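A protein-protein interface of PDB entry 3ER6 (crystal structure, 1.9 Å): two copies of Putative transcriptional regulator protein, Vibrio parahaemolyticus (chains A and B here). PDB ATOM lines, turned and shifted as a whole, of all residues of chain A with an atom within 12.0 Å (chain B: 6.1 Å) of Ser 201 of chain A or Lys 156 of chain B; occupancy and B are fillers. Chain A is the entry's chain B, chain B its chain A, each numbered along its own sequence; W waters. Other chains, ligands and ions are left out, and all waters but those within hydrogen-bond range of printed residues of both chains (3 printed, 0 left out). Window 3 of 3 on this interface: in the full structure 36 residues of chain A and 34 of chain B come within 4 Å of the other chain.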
ATOM      1  N   ILE A  30       0.630  -0.534 -21.397  1.00  0.00           N
ATOM      2  CA  ILE A  30       1.767  -0.923 -20.527  1.00  0.00           C
ATOM      3  C   ILE A  30       3.075  -0.801 -21.288  1.00  0.00           C
ATOM      4  O   ILE A  30       4.002  -0.125 -20.850  1.00  0.00           O
ATOM      5  CB  ILE A  30       1.568  -2.367 -19.966  1.00  0.00           C
ATOM      6  CG1 ILE A  30       0.361  -2.364 -18.983  1.00  0.00           C
ATOM      7  CG2 ILE A  30       2.934  -2.924 -19.353  1.00  0.00           C
ATOM      8  CD1 ILE A  30      -0.138  -3.757 -18.548  1.00  0.00           C
ATOM      9  N   TYR A 170      -7.378 -10.586 -17.875  1.00  0.00           N
ATOM     10  CA  TYR A 170      -7.013  -9.179 -17.859  1.00  0.00           C
ATOM     11  C   TYR A 170      -5.668  -8.802 -17.241  1.00  0.00           C
ATOM     12  O   TYR A 170      -5.176  -7.648 -17.441  1.00  0.00           O
ATOM     13  CB  TYR A 170      -8.117  -8.326 -17.228  1.00  0.00           C
ATOM     14  CG  TYR A 170      -9.405  -8.457 -18.002  1.00  0.00           C
ATOM     15  CD1 TYR A 170      -9.536  -7.886 -19.279  1.00  0.00           C
ATOM     16  CD2 TYR A 170     -10.484  -9.189 -17.470  1.00  0.00           C
ATOM     17  CE1 TYR A 170     -10.721  -8.018 -19.986  1.00  0.00           C
ATOM     18  CE2 TYR A 170     -11.640  -9.363 -18.179  1.00  0.00           C
ATOM     19  CZ  TYR A 170     -11.757  -8.745 -19.423  1.00  0.00           C
ATOM     20  OH  TYR A 170     -12.901  -8.907 -20.132  1.00  0.00           O
ATOM     21  N   SER A 171      -5.075  -9.730 -16.495  1.00  0.00           N
ATOM     22  CA  SER A 171      -3.810  -9.419 -15.900  1.00  0.00           C
ATOM     23  C   SER A 171      -2.713 -10.232 -16.551  1.00  0.00           C
ATOM     24  O   SER A 171      -2.640 -11.454 -16.432  1.00  0.00           O
ATOM     25  CB  SER A 171      -3.833  -9.566 -14.390  1.00  0.00           C
ATOM     26  OG  SER A 171      -4.069 -10.912 -14.059  1.00  0.00           O
ATOM     27  N   HIS A 172      -1.921  -9.518 -17.335  1.00  0.00           N
ATOM     28  CA  HIS A 172      -0.877 -10.103 -18.140  1.00  0.00           C
ATOM     29  C   HIS A 172       0.454  -9.475 -17.724  1.00  0.00           C
ATOM     30  O   HIS A 172       1.385  -9.347 -18.540  1.00  0.00           O
ATOM     31  CB  HIS A 172      -1.194  -9.946 -19.632  1.00  0.00           C
ATOM     32  CG  HIS A 172      -2.548 -10.481 -20.008  1.00  0.00           C
ATOM     33  ND1 HIS A 172      -2.830 -11.823 -20.076  1.00  0.00           N
ATOM     34  CD2 HIS A 172      -3.728  -9.841 -20.240  1.00  0.00           C
ATOM     35  CE1 HIS A 172      -4.112 -12.000 -20.372  1.00  0.00           C
ATOM     36  NE2 HIS A 172      -4.688 -10.809 -20.446  1.00  0.00           N
ATOM     37  N   SER A 173       0.579  -9.171 -16.430  1.00  0.00           N
ATOM     38  CA  SER A 173       1.739  -8.419 -15.961  1.00  0.00           C
ATOM     39  C   SER A 173       3.031  -9.208 -16.128  1.00  0.00           C
ATOM     40  O   SER A 173       4.042  -8.624 -16.535  1.00  0.00           O
ATOM     41  CB  SER A 173       1.573  -7.945 -14.506  1.00  0.00           C
ATOM     42  OG  SER A 173       1.460  -9.068 -13.632  1.00  0.00           O
ATOM     43  N   SER A 174       3.026 -10.516 -15.852  1.00  0.00           N
ATOM     44  CA  SER A 174       4.294 -11.221 -15.906  1.00  0.00           C
ATOM     45  C   SER A 174       4.879 -11.283 -17.320  1.00  0.00           C
ATOM     46  O   SER A 174       6.073 -11.041 -17.494  1.00  0.00           O
ATOM     47  CB  SER A 174       4.247 -12.626 -15.263  1.00  0.00           C
ATOM     48  OG  SER A 174       3.196 -13.390 -15.846  1.00  0.00           O
ATOM     49  N   VAL A 175       4.059 -11.630 -18.307  1.00  0.00           N
ATOM     50  CA  VAL A 175       4.525 -11.641 -19.699  1.00  0.00           C
ATOM     51  C   VAL A 175       4.906 -10.224 -20.177  1.00  0.00           C
ATOM     52  O   VAL A 175       5.929 -10.042 -20.825  1.00  0.00           O
ATOM     53  CB  VAL A 175       3.455 -12.302 -20.609  1.00  0.00           C
ATOM     54  CG1 VAL A 175       3.650 -11.989 -22.086  1.00  0.00           C
ATOM     55  CG2 VAL A 175       3.423 -13.844 -20.366  1.00  0.00           C
ATOM     56  N   MET A 176       4.085  -9.219 -19.872  1.00  0.00           N
ATOM     57  CA  MET A 176       4.416  -7.866 -20.318  1.00  0.00           C
ATOM     58  C   MET A 176       5.754  -7.378 -19.736  1.00  0.00           C
ATOM     59  O   MET A 176       6.579  -6.785 -20.446  1.00  0.00           O
ATOM     60  CB  MET A 176       3.301  -6.887 -19.970  1.00  0.00           C
ATOM     61  CG  MET A 176       2.029  -7.126 -20.808  1.00  0.00           C
ATOM     62  SD  MET A 176       2.247  -6.842 -22.583  1.00  0.00           S
ATOM     63  CE  MET A 176       2.078  -8.218 -23.318  1.00  0.00           C
ATOM     64  N   LEU A 177       5.937  -7.559 -18.436  1.00  0.00           N
ATOM     65  CA  LEU A 177       7.170  -7.139 -17.785  1.00  0.00           C
ATOM     66  C   LEU A 177       8.398  -7.945 -18.285  1.00  0.00           C
ATOM     67  O   LEU A 177       9.515  -7.408 -18.386  1.00  0.00           O
ATOM     68  CB  LEU A 177       7.013  -7.287 -16.260  1.00  0.00           C
ATOM     69  CG  LEU A 177       5.953  -6.334 -15.692  1.00  0.00           C
ATOM     70  CD1 LEU A 177       5.884  -6.475 -14.152  1.00  0.00           C
ATOM     71  CD2 LEU A 177       6.332  -4.937 -16.090  1.00  0.00           C
ATOM     72  N   GLU A 178       8.202  -9.222 -18.561  1.00  0.00           N
ATOM     73  CA  GLU A 178       9.271 -10.031 -19.164  1.00  0.00           C
ATOM     74  C   GLU A 178       9.736  -9.370 -20.462  1.00  0.00           C
ATOM     75  O   GLU A 178      10.934  -9.184 -20.677  1.00  0.00           O
ATOM     76  CB  GLU A 178       8.756 -11.432 -19.541  1.00  0.00           C
ATOM     77  CG  GLU A 178       9.133 -12.479 -18.575  1.00  0.00           C
ATOM     78  CD  GLU A 178      10.584 -12.843 -18.750  1.00  0.00           C
ATOM     79  OE1 GLU A 178      10.882 -13.696 -19.619  1.00  0.00           O
ATOM     80  OE2 GLU A 178      11.428 -12.257 -18.037  1.00  0.00           O
ATOM     81  N   GLN A 194       8.808   2.925 -10.006  1.00  0.00           N
ATOM     82  CA  GLN A 194       7.500   2.842  -9.363  1.00  0.00           C
ATOM     83  C   GLN A 194       6.451   2.394 -10.379  1.00  0.00           C
ATOM     84  O   GLN A 194       5.483   1.697 -10.021  1.00  0.00           O
ATOM     85  CB  GLN A 194       7.120   4.181  -8.748  1.00  0.00           C
ATOM     86  CG  GLN A 194       7.721   4.357  -7.325  1.00  0.00           C
ATOM     87  CD  GLN A 194       8.176   5.805  -6.999  1.00  0.00           C
ATOM     88  OE1 GLN A 194       8.655   6.081  -5.882  1.00  0.00           O
ATOM     89  NE2 GLN A 194       8.034   6.723  -7.967  1.00  0.00           N
ATOM     90  N   PHE A 195       6.662   2.762 -11.641  1.00  0.00           N
ATOM     91  CA  PHE A 195       5.704   2.359 -12.644  1.00  0.00           C
ATOM     92  C   PHE A 195       5.742   0.834 -12.780  1.00  0.00           C
ATOM     93  O   PHE A 195       4.710   0.168 -12.744  1.00  0.00           O
ATOM     94  CB  PHE A 195       5.928   3.028 -14.011  1.00  0.00           C
ATOM     95  CG  PHE A 195       5.087   2.411 -15.099  1.00  0.00           C
ATOM     96  CD1 PHE A 195       3.695   2.587 -15.099  1.00  0.00           C
ATOM     97  CD2 PHE A 195       5.666   1.581 -16.062  1.00  0.00           C
ATOM     98  CE1 PHE A 195       2.902   1.986 -16.075  1.00  0.00           C
ATOM     99  CE2 PHE A 195       4.872   0.965 -17.042  1.00  0.00           C
ATOM    100  CZ  PHE A 195       3.507   1.164 -17.050  1.00  0.00           C
ATOM    101  N   LEU A 196       6.953   0.281 -12.923  1.00  0.00           N
ATOM    102  CA  LEU A 196       7.097  -1.159 -13.174  1.00  0.00           C
ATOM    103  C   LEU A 196       6.599  -1.956 -11.958  1.00  0.00           C
ATOM    104  O   LEU A 196       5.992  -2.999 -12.072  1.00  0.00           O
ATOM    105  CB  LEU A 196       8.529  -1.529 -13.627  1.00  0.00           C
ATOM    106  CG  LEU A 196       8.738  -0.923 -15.059  1.00  0.00           C
ATOM    107  CD1 LEU A 196      10.159  -1.101 -15.691  1.00  0.00           C
ATOM    108  CD2 LEU A 196       7.632  -1.312 -16.101  1.00  0.00           C
ATOM    109  N   SER A 197       6.796  -1.377 -10.787  1.00  0.00           N
ATOM    110  CA  SER A 197       6.357  -1.955  -9.585  1.00  0.00           C
ATOM    111  C   SER A 197       4.844  -1.899  -9.438  1.00  0.00           C
ATOM    112  O   SER A 197       4.232  -2.808  -8.897  1.00  0.00           O
ATOM    113  CB  SER A 197       7.015  -1.189  -8.448  1.00  0.00           C
ATOM    114  OG  SER A 197       6.734  -1.880  -7.261  1.00  0.00           O
ATOM    115  N   THR A 198       4.246  -0.819  -9.925  1.00  0.00           N
ATOM    116  CA  THR A 198       2.783  -0.655  -9.912  1.00  0.00           C
ATOM    117  C   THR A 198       2.112  -1.738 -10.776  1.00  0.00           C
ATOM    118  O   THR A 198       1.123  -2.357 -10.388  1.00  0.00           O
ATOM    119  CB  THR A 198       2.409   0.756 -10.372  1.00  0.00           C
ATOM    120  OG1 THR A 198       2.749   1.697  -9.352  1.00  0.00           O
ATOM    121  CG2 THR A 198       0.932   0.880 -10.611  1.00  0.00           C
ATOM    122  N   ILE A 199       2.716  -2.009 -11.917  1.00  0.00           N
ATOM    123  CA  ILE A 199       2.241  -3.071 -12.790  1.00  0.00           C
ATOM    124  C   ILE A 199       2.441  -4.432 -12.165  1.00  0.00           C
ATOM    125  O   ILE A 199       1.532  -5.264 -12.107  1.00  0.00           O
ATOM    126  CB  ILE A 199       2.980  -3.017 -14.160  1.00  0.00           C
ATOM    127  CG1 ILE A 199       2.681  -1.703 -14.868  1.00  0.00           C
ATOM    128  CG2 ILE A 199       2.572  -4.230 -15.033  1.00  0.00           C
ATOM    129  CD1 ILE A 199       1.171  -1.410 -15.031  1.00  0.00           C
ATOM    130  N   GLU A 200       3.653  -4.690 -11.690  1.00  0.00           N
ATOM    131  CA  GLU A 200       3.949  -6.004 -11.126  1.00  0.00           C
ATOM    132  C   GLU A 200       3.138  -6.323  -9.870  1.00  0.00           C
ATOM    133  O   GLU A 200       2.745  -7.480  -9.646  1.00  0.00           O
ATOM    134  CB  GLU A 200       5.453  -6.065 -10.837  1.00  0.00           C
ATOM    135  CG  GLU A 200       5.937  -7.408 -10.476  1.00  0.00           C
ATOM    136  CD  GLU A 200       7.450  -7.477 -10.612  1.00  0.00           C
ATOM    137  OE1 GLU A 200       8.138  -6.570 -10.073  1.00  0.00           O
ATOM    138  OE2 GLU A 200       7.917  -8.432 -11.282  1.00  0.00           O
ATOM    139  N   SER A 201       2.852  -5.310  -9.047  1.00  0.00           N
ATOM    140  CA  SER A 201       2.156  -5.562  -7.807  1.00  0.00           C
ATOM    141  C   SER A 201       0.748  -6.151  -8.020  1.00  0.00           C
ATOM    142  O   SER A 201       0.216  -6.794  -7.130  1.00  0.00           O
ATOM    143  CB  SER A 201       2.089  -4.292  -6.938  1.00  0.00           C
ATOM    144  OG  SER A 201       1.271  -3.310  -7.548  1.00  0.00           O
ATOM    145  N   GLU A 202       0.150  -5.919  -9.189  1.00  0.00           N
ATOM    146  CA  GLU A 202      -1.183  -6.457  -9.470  1.00  0.00           C
ATOM    147  C   GLU A 202      -1.111  -7.950  -9.852  1.00  0.00           C
ATOM    148  O   GLU A 202      -2.122  -8.585 -10.033  1.00  0.00           O
ATOM    149  CB  GLU A 202      -1.868  -5.681 -10.620  1.00  0.00           C
ATOM    150  CG  GLU A 202      -1.895  -4.128 -10.547  1.00  0.00           C
ATOM    151  CD  GLU A 202      -2.957  -3.571 -11.510  1.00  0.00           C
ATOM    152  OE1 GLU A 202      -4.137  -3.608 -11.101  1.00  0.00           O
ATOM    153  OE2 GLU A 202      -2.641  -3.159 -12.675  1.00  0.00           O
ATOM    154  N   GLY A 203       0.077  -8.493 -10.067  1.00  0.00           N
ATOM    155  CA  GLY A 203       0.229  -9.938 -10.205  1.00  0.00           C
ATOM    156  C   GLY A 203       0.123 -10.533  -8.799  1.00  0.00           C
ATOM    157  O   GLY A 203       0.244 -11.751  -8.614  1.00  0.00           O
ATOM    158  N   VAL B 133      -7.398   5.248  -1.742  1.00  0.00           N
ATOM    159  CA  VAL B 133      -6.298   4.346  -2.120  1.00  0.00           C
ATOM    160  C   VAL B 133      -5.627   4.883  -3.399  1.00  0.00           C
ATOM    161  O   VAL B 133      -6.278   5.498  -4.227  1.00  0.00           O
ATOM    162  CB  VAL B 133      -6.859   2.903  -2.357  1.00  0.00           C
ATOM    163  CG1 VAL B 133      -7.422   2.327  -1.044  1.00  0.00           C
ATOM    164  CG2 VAL B 133      -7.955   2.892  -3.486  1.00  0.00           C
ATOM    165  N   HIS B 135      -2.251   3.696  -6.325  1.00  0.00           N
ATOM    166  CA  HIS B 135      -1.115   2.820  -6.550  1.00  0.00           C
ATOM    167  C   HIS B 135       0.190   3.625  -6.367  1.00  0.00           C
ATOM    168  O   HIS B 135       0.184   4.882  -6.302  1.00  0.00           O
ATOM    169  CB  HIS B 135      -1.192   2.134  -7.936  1.00  0.00           C
ATOM    170  CG  HIS B 135      -1.492   3.070  -9.061  1.00  0.00           C
ATOM    171  ND1 HIS B 135      -0.641   4.082  -9.430  1.00  0.00           N
ATOM    172  CD2 HIS B 135      -2.583   3.176  -9.873  1.00  0.00           C
ATOM    173  CE1 HIS B 135      -1.178   4.758 -10.435  1.00  0.00           C
ATOM    174  NE2 HIS B 135      -2.356   4.231 -10.717  1.00  0.00           N
ATOM    175  N   MET B 152      -4.857   4.627   2.306  1.00  0.00           N
ATOM    176  CA  MET B 152      -4.866   3.376   3.012  1.00  0.00           C
ATOM    177  C   MET B 152      -3.874   2.510   2.272  1.00  0.00           C
ATOM    178  O   MET B 152      -4.182   1.902   1.248  1.00  0.00           O
ATOM    179  CB  MET B 152      -6.260   2.806   2.986  1.00  0.00           C
ATOM    180  CG  MET B 152      -7.262   3.759   3.622  1.00  0.00           C
ATOM    181  SD  MET B 152      -6.813   4.335   5.309  1.00  0.00           S
ATOM    182  CE  MET B 152      -7.229   2.851   6.161  1.00  0.00           C
ATOM    183  N   GLU B 154      -2.272  -0.242   2.574  1.00  0.00           N
ATOM    184  CA  GLU B 154      -2.281  -1.677   2.399  1.00  0.00           C
ATOM    185  C   GLU B 154      -3.569  -2.198   1.744  1.00  0.00           C
ATOM    186  O   GLU B 154      -3.881  -3.375   1.878  1.00  0.00           O
ATOM    187  CB  GLU B 154      -2.099  -2.353   3.751  1.00  0.00           C
ATOM    188  CG  GLU B 154      -0.773  -2.021   4.437  1.00  0.00           C
ATOM    189  CD  GLU B 154      -0.818  -2.439   5.889  1.00  0.00           C
ATOM    190  OE1 GLU B 154      -1.816  -2.070   6.569  1.00  0.00           O
ATOM    191  OE2 GLU B 154       0.111  -3.162   6.338  1.00  0.00           O
ATOM    192  N   GLN B 155      -4.326  -1.324   1.079  1.00  0.00           N
ATOM    193  CA  GLN B 155      -5.495  -1.746   0.342  1.00  0.00           C
ATOM    194  C   GLN B 155      -5.382  -1.340  -1.131  1.00  0.00           C
ATOM    195  O   GLN B 155      -4.762  -0.319  -1.442  1.00  0.00           O
ATOM    196  CB  GLN B 155      -6.724  -1.055   0.886  1.00  0.00           C
ATOM    197  CG  GLN B 155      -7.218  -1.605   2.157  1.00  0.00           C
ATOM    198  CD  GLN B 155      -8.139  -0.620   2.812  1.00  0.00           C
ATOM    199  OE1 GLN B 155      -7.876  -0.191   3.930  1.00  0.00           O
ATOM    200  NE2 GLN B 155      -9.181  -0.186   2.093  1.00  0.00           N
ATOM    201  N   LYS B 156      -6.019  -2.106  -2.022  1.00  0.00           N
ATOM    202  CA  LYS B 156      -5.968  -1.781  -3.468  1.00  0.00           C
ATOM    203  C   LYS B 156      -7.334  -1.265  -3.849  1.00  0.00           C
ATOM    204  O   LYS B 156      -7.573  -0.847  -4.997  1.00  0.00           O
ATOM    205  CB  LYS B 156      -5.702  -3.048  -4.312  1.00  0.00           C
ATOM    206  CG  LYS B 156      -4.262  -3.653  -4.250  1.00  0.00           C
ATOM    207  CD  LYS B 156      -4.310  -5.154  -4.704  1.00  0.00           C
ATOM    208  CE  LYS B 156      -3.059  -5.723  -5.457  1.00  0.00           C
ATOM    209  NZ  LYS B 156      -1.685  -5.529  -4.891  1.00  0.00           N
ATOM    210  N   ALA B 157      -8.270  -1.391  -2.914  1.00  0.00           N
ATOM    211  CA  ALA B 157      -9.624  -0.943  -3.153  1.00  0.00           C
ATOM    212  C   ALA B 157     -10.240  -0.441  -1.843  1.00  0.00           C
ATOM    213  O   ALA B 157      -9.809  -0.831  -0.737  1.00  0.00           O
ATOM    214  CB  ALA B 157     -10.467  -2.060  -3.762  1.00  0.00           C
ATOM    215  N   LEU B 158     -11.271   0.374  -1.959  1.00  0.00           N
ATOM    216  CA  LEU B 158     -11.958   0.926  -0.746  1.00  0.00           C
ATOM    217  C   LEU B 158     -13.365   1.321  -1.102  1.00  0.00           C
ATOM    218  O   LEU B 158     -13.585   1.887  -2.196  1.00  0.00           O
ATOM    219  CB  LEU B 158     -11.212   2.184  -0.282  1.00  0.00           C
ATOM    220  CG  LEU B 158     -11.704   3.073   0.870  1.00  0.00           C
ATOM    221  CD1 LEU B 158     -10.482   3.742   1.508  1.00  0.00           C
ATOM    222  CD2 LEU B 158     -12.696   4.147   0.440  1.00  0.00           C
ATOM    223  N   LEU B 165     -13.628   2.763  -4.870  1.00  0.00           N
ATOM    224  CA  LEU B 165     -12.351   3.107  -5.383  1.00  0.00           C
ATOM    225  C   LEU B 165     -11.508   1.848  -5.667  1.00  0.00           C
ATOM    226  O   LEU B 165     -11.380   0.942  -4.809  1.00  0.00           O
ATOM    227  CB  LEU B 165     -11.535   3.966  -4.371  1.00  0.00           C
ATOM    228  CG  LEU B 165     -12.167   5.240  -3.762  1.00  0.00           C
ATOM    229  CD1 LEU B 165     -11.119   5.920  -2.840  1.00  0.00           C
ATOM    230  CD2 LEU B 165     -12.652   6.222  -4.857  1.00  0.00           C
ATOM    231  N   SER B 166     -10.899   1.804  -6.853  1.00  0.00           N
ATOM    232  CA  SER B 166     -10.041   0.674  -7.195  1.00  0.00           C
ATOM    233  C   SER B 166      -8.741   1.232  -7.900  1.00  0.00           C
ATOM    234  O   SER B 166      -8.805   1.715  -9.028  1.00  0.00           O
ATOM    235  CB  SER B 166     -10.783  -0.340  -8.084  1.00  0.00           C
ATOM    236  OG  SER B 166      -9.850  -1.350  -8.513  1.00  0.00           O
ATOM    237  N   SER B 167      -7.599   1.195  -7.200  1.00  0.00           N
ATOM    238  CA  SER B 167      -6.303   1.718  -7.706  1.00  0.00           C
ATOM    239  C   SER B 167      -5.909   1.165  -9.084  1.00  0.00           C
ATOM    240  O   SER B 167      -5.508   1.898  -9.965  1.00  0.00           O
ATOM    241  CB  SER B 167      -5.163   1.374  -6.738  1.00  0.00           C
ATOM    242  OG  SER B 167      -5.337   2.100  -5.551  1.00  0.00           O
ATOM    243  N   GLY B 168      -6.015  -0.142  -9.242  1.00  0.00           N
ATOM    244  CA  GLY B 168      -5.544  -0.796 -10.433  1.00  0.00           C
ATOM    245  C   GLY B 168      -4.030  -0.621 -10.575  1.00  0.00           C
ATOM    246  O   GLY B 168      -3.276  -0.757  -9.579  1.00  0.00           O
ATOM    247  N   SER B 171      -6.232  -4.158 -12.692  1.00  0.00           N
ATOM    248  CA  SER B 171      -6.964  -5.164 -11.939  1.00  0.00           C
ATOM    249  C   SER B 171      -8.006  -4.524 -11.043  1.00  0.00           C
ATOM    250  O   SER B 171      -7.648  -3.838 -10.077  1.00  0.00           O
ATOM    251  CB  SER B 171      -6.000  -6.004 -11.092  1.00  0.00           C
ATOM    252  OG  SER B 171      -5.415  -7.010 -11.887  1.00  0.00           O
ATOM    253  N   SER B 174     -11.901  -6.889  -7.337  1.00  0.00           N
ATOM    254  CA  SER B 174     -12.639  -6.870  -6.095  1.00  0.00           C
ATOM    255  C   SER B 174     -13.834  -5.900  -6.175  1.00  0.00           C
ATOM    256  O   SER B 174     -14.943  -6.250  -5.746  1.00  0.00           O
ATOM    257  CB  SER B 174     -11.772  -6.651  -4.850  1.00  0.00           C
ATOM    258  OG  SER B 174     -11.369  -5.307  -4.767  1.00  0.00           O
HETATM  259  O   HOH W   1      -0.627  -1.296  -8.669  1.00  0.00           O
HETATM  260  O   HOH W   2      -4.996  -3.959  -8.309  1.00  0.00           O
HETATM  261  O   HOH W   3      -1.464  -3.512  -6.726  1.00  0.00           O
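Ser 171 of chain A touches its own counterpart, Ser 171 of chain B.
2 positions are printed for both chains.
Of the 5 pairs that touch across the chains among the printed residues, 1 has its exchanged pair printed and touching as well.
Among the printed residues, pairs that only touch across the chains: Ser 171 of chain A with Ser 171 of chain B and Thr 198 of chain A with His 135 of chain B.
The side-chain hydroxyl (OG1) of Thr 198 of chain A is in hydrogen-bond range of the backbone carbonyl oxygen (O) of Gln 194 of chain A (2.8 Å).
O of Thr 198 of chain A lies within hydrogen-bond range of OG of Ser 201 of chain A, 3.0 Å away.
The side-chain hydroxyl (OG) of Ser 201 of chain A lies close to the backbone carbonyl oxygen (O) of Ser 197 of chain A (3.3 Å).
O of Lys 156 of chain B lies within hydrogen-bond range of N of Ser 167 of chain B (3.0 Å).
Hydrophobic or aromatic side chains of chain B that line the printed part of chain A: His 135.
Of the 20 printed residues of chain A, 4 touch a printed residue of chain B.
Among the printed residues, 5 pairs touch across the chains.
Among the printed residues, no Asp or Glu carboxylate lies within 4 Å of a Lys or Arg side-chain nitrogen of the other chain.
Water W1 lies within hydrogen-bond range of the backbone carbonyl oxygen of Thr 198 of chain A, the backbone carbonyl oxygen of Gly 168 of chain B and the side-chain hydroxyl of Ser 201 of chain A.
Water W3 bridges the side-chain amino group of Lys 156 of chain B (2.7 Å) and the side-chain hydroxyl of Ser 201 of chain A (2.9 Å).
Water W2 bridges OE1 of Glu 202 of chain A (2.9 Å) and O of Ser 171 of chain B (3.2 Å).
Of the printed residues of chain B, Thr 198 of chain A touches His 135.
Ser 201 of chain A touches just one residue of chain B: Lys 156.
Gly 203 of chain A touches none of the printed residues of chain B.
No residue of chain A comes within 4 Å of Gln 155 of chain B.
No residue of chain A comes within 4 Å of Ala 157 of chain B.
No residue of chain A comes within 4 Å of Ser 167 of chain B.
Printed residues of chain A within 4 Å of Ser 171 of chain B: Ser 171 (3.9 Å) and Glu 202 (2.7 Å).
The backbone carbonyl oxygen (O) of Gly 168 of chain B sits close to the side-chain carboxylate (OE1) of Glu 202 of chain A (3.3 Å).
The backbone carbonyl oxygen of Ser 201 of chain A is in hydrogen-bond range of the side-chain amino group of Lys 156 of chain B, at 3.2 Å.
N of Ser 171 of chain B lies within hydrogen-bond range of OE1 of Glu 202 of chain A, at 2.7 Å.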
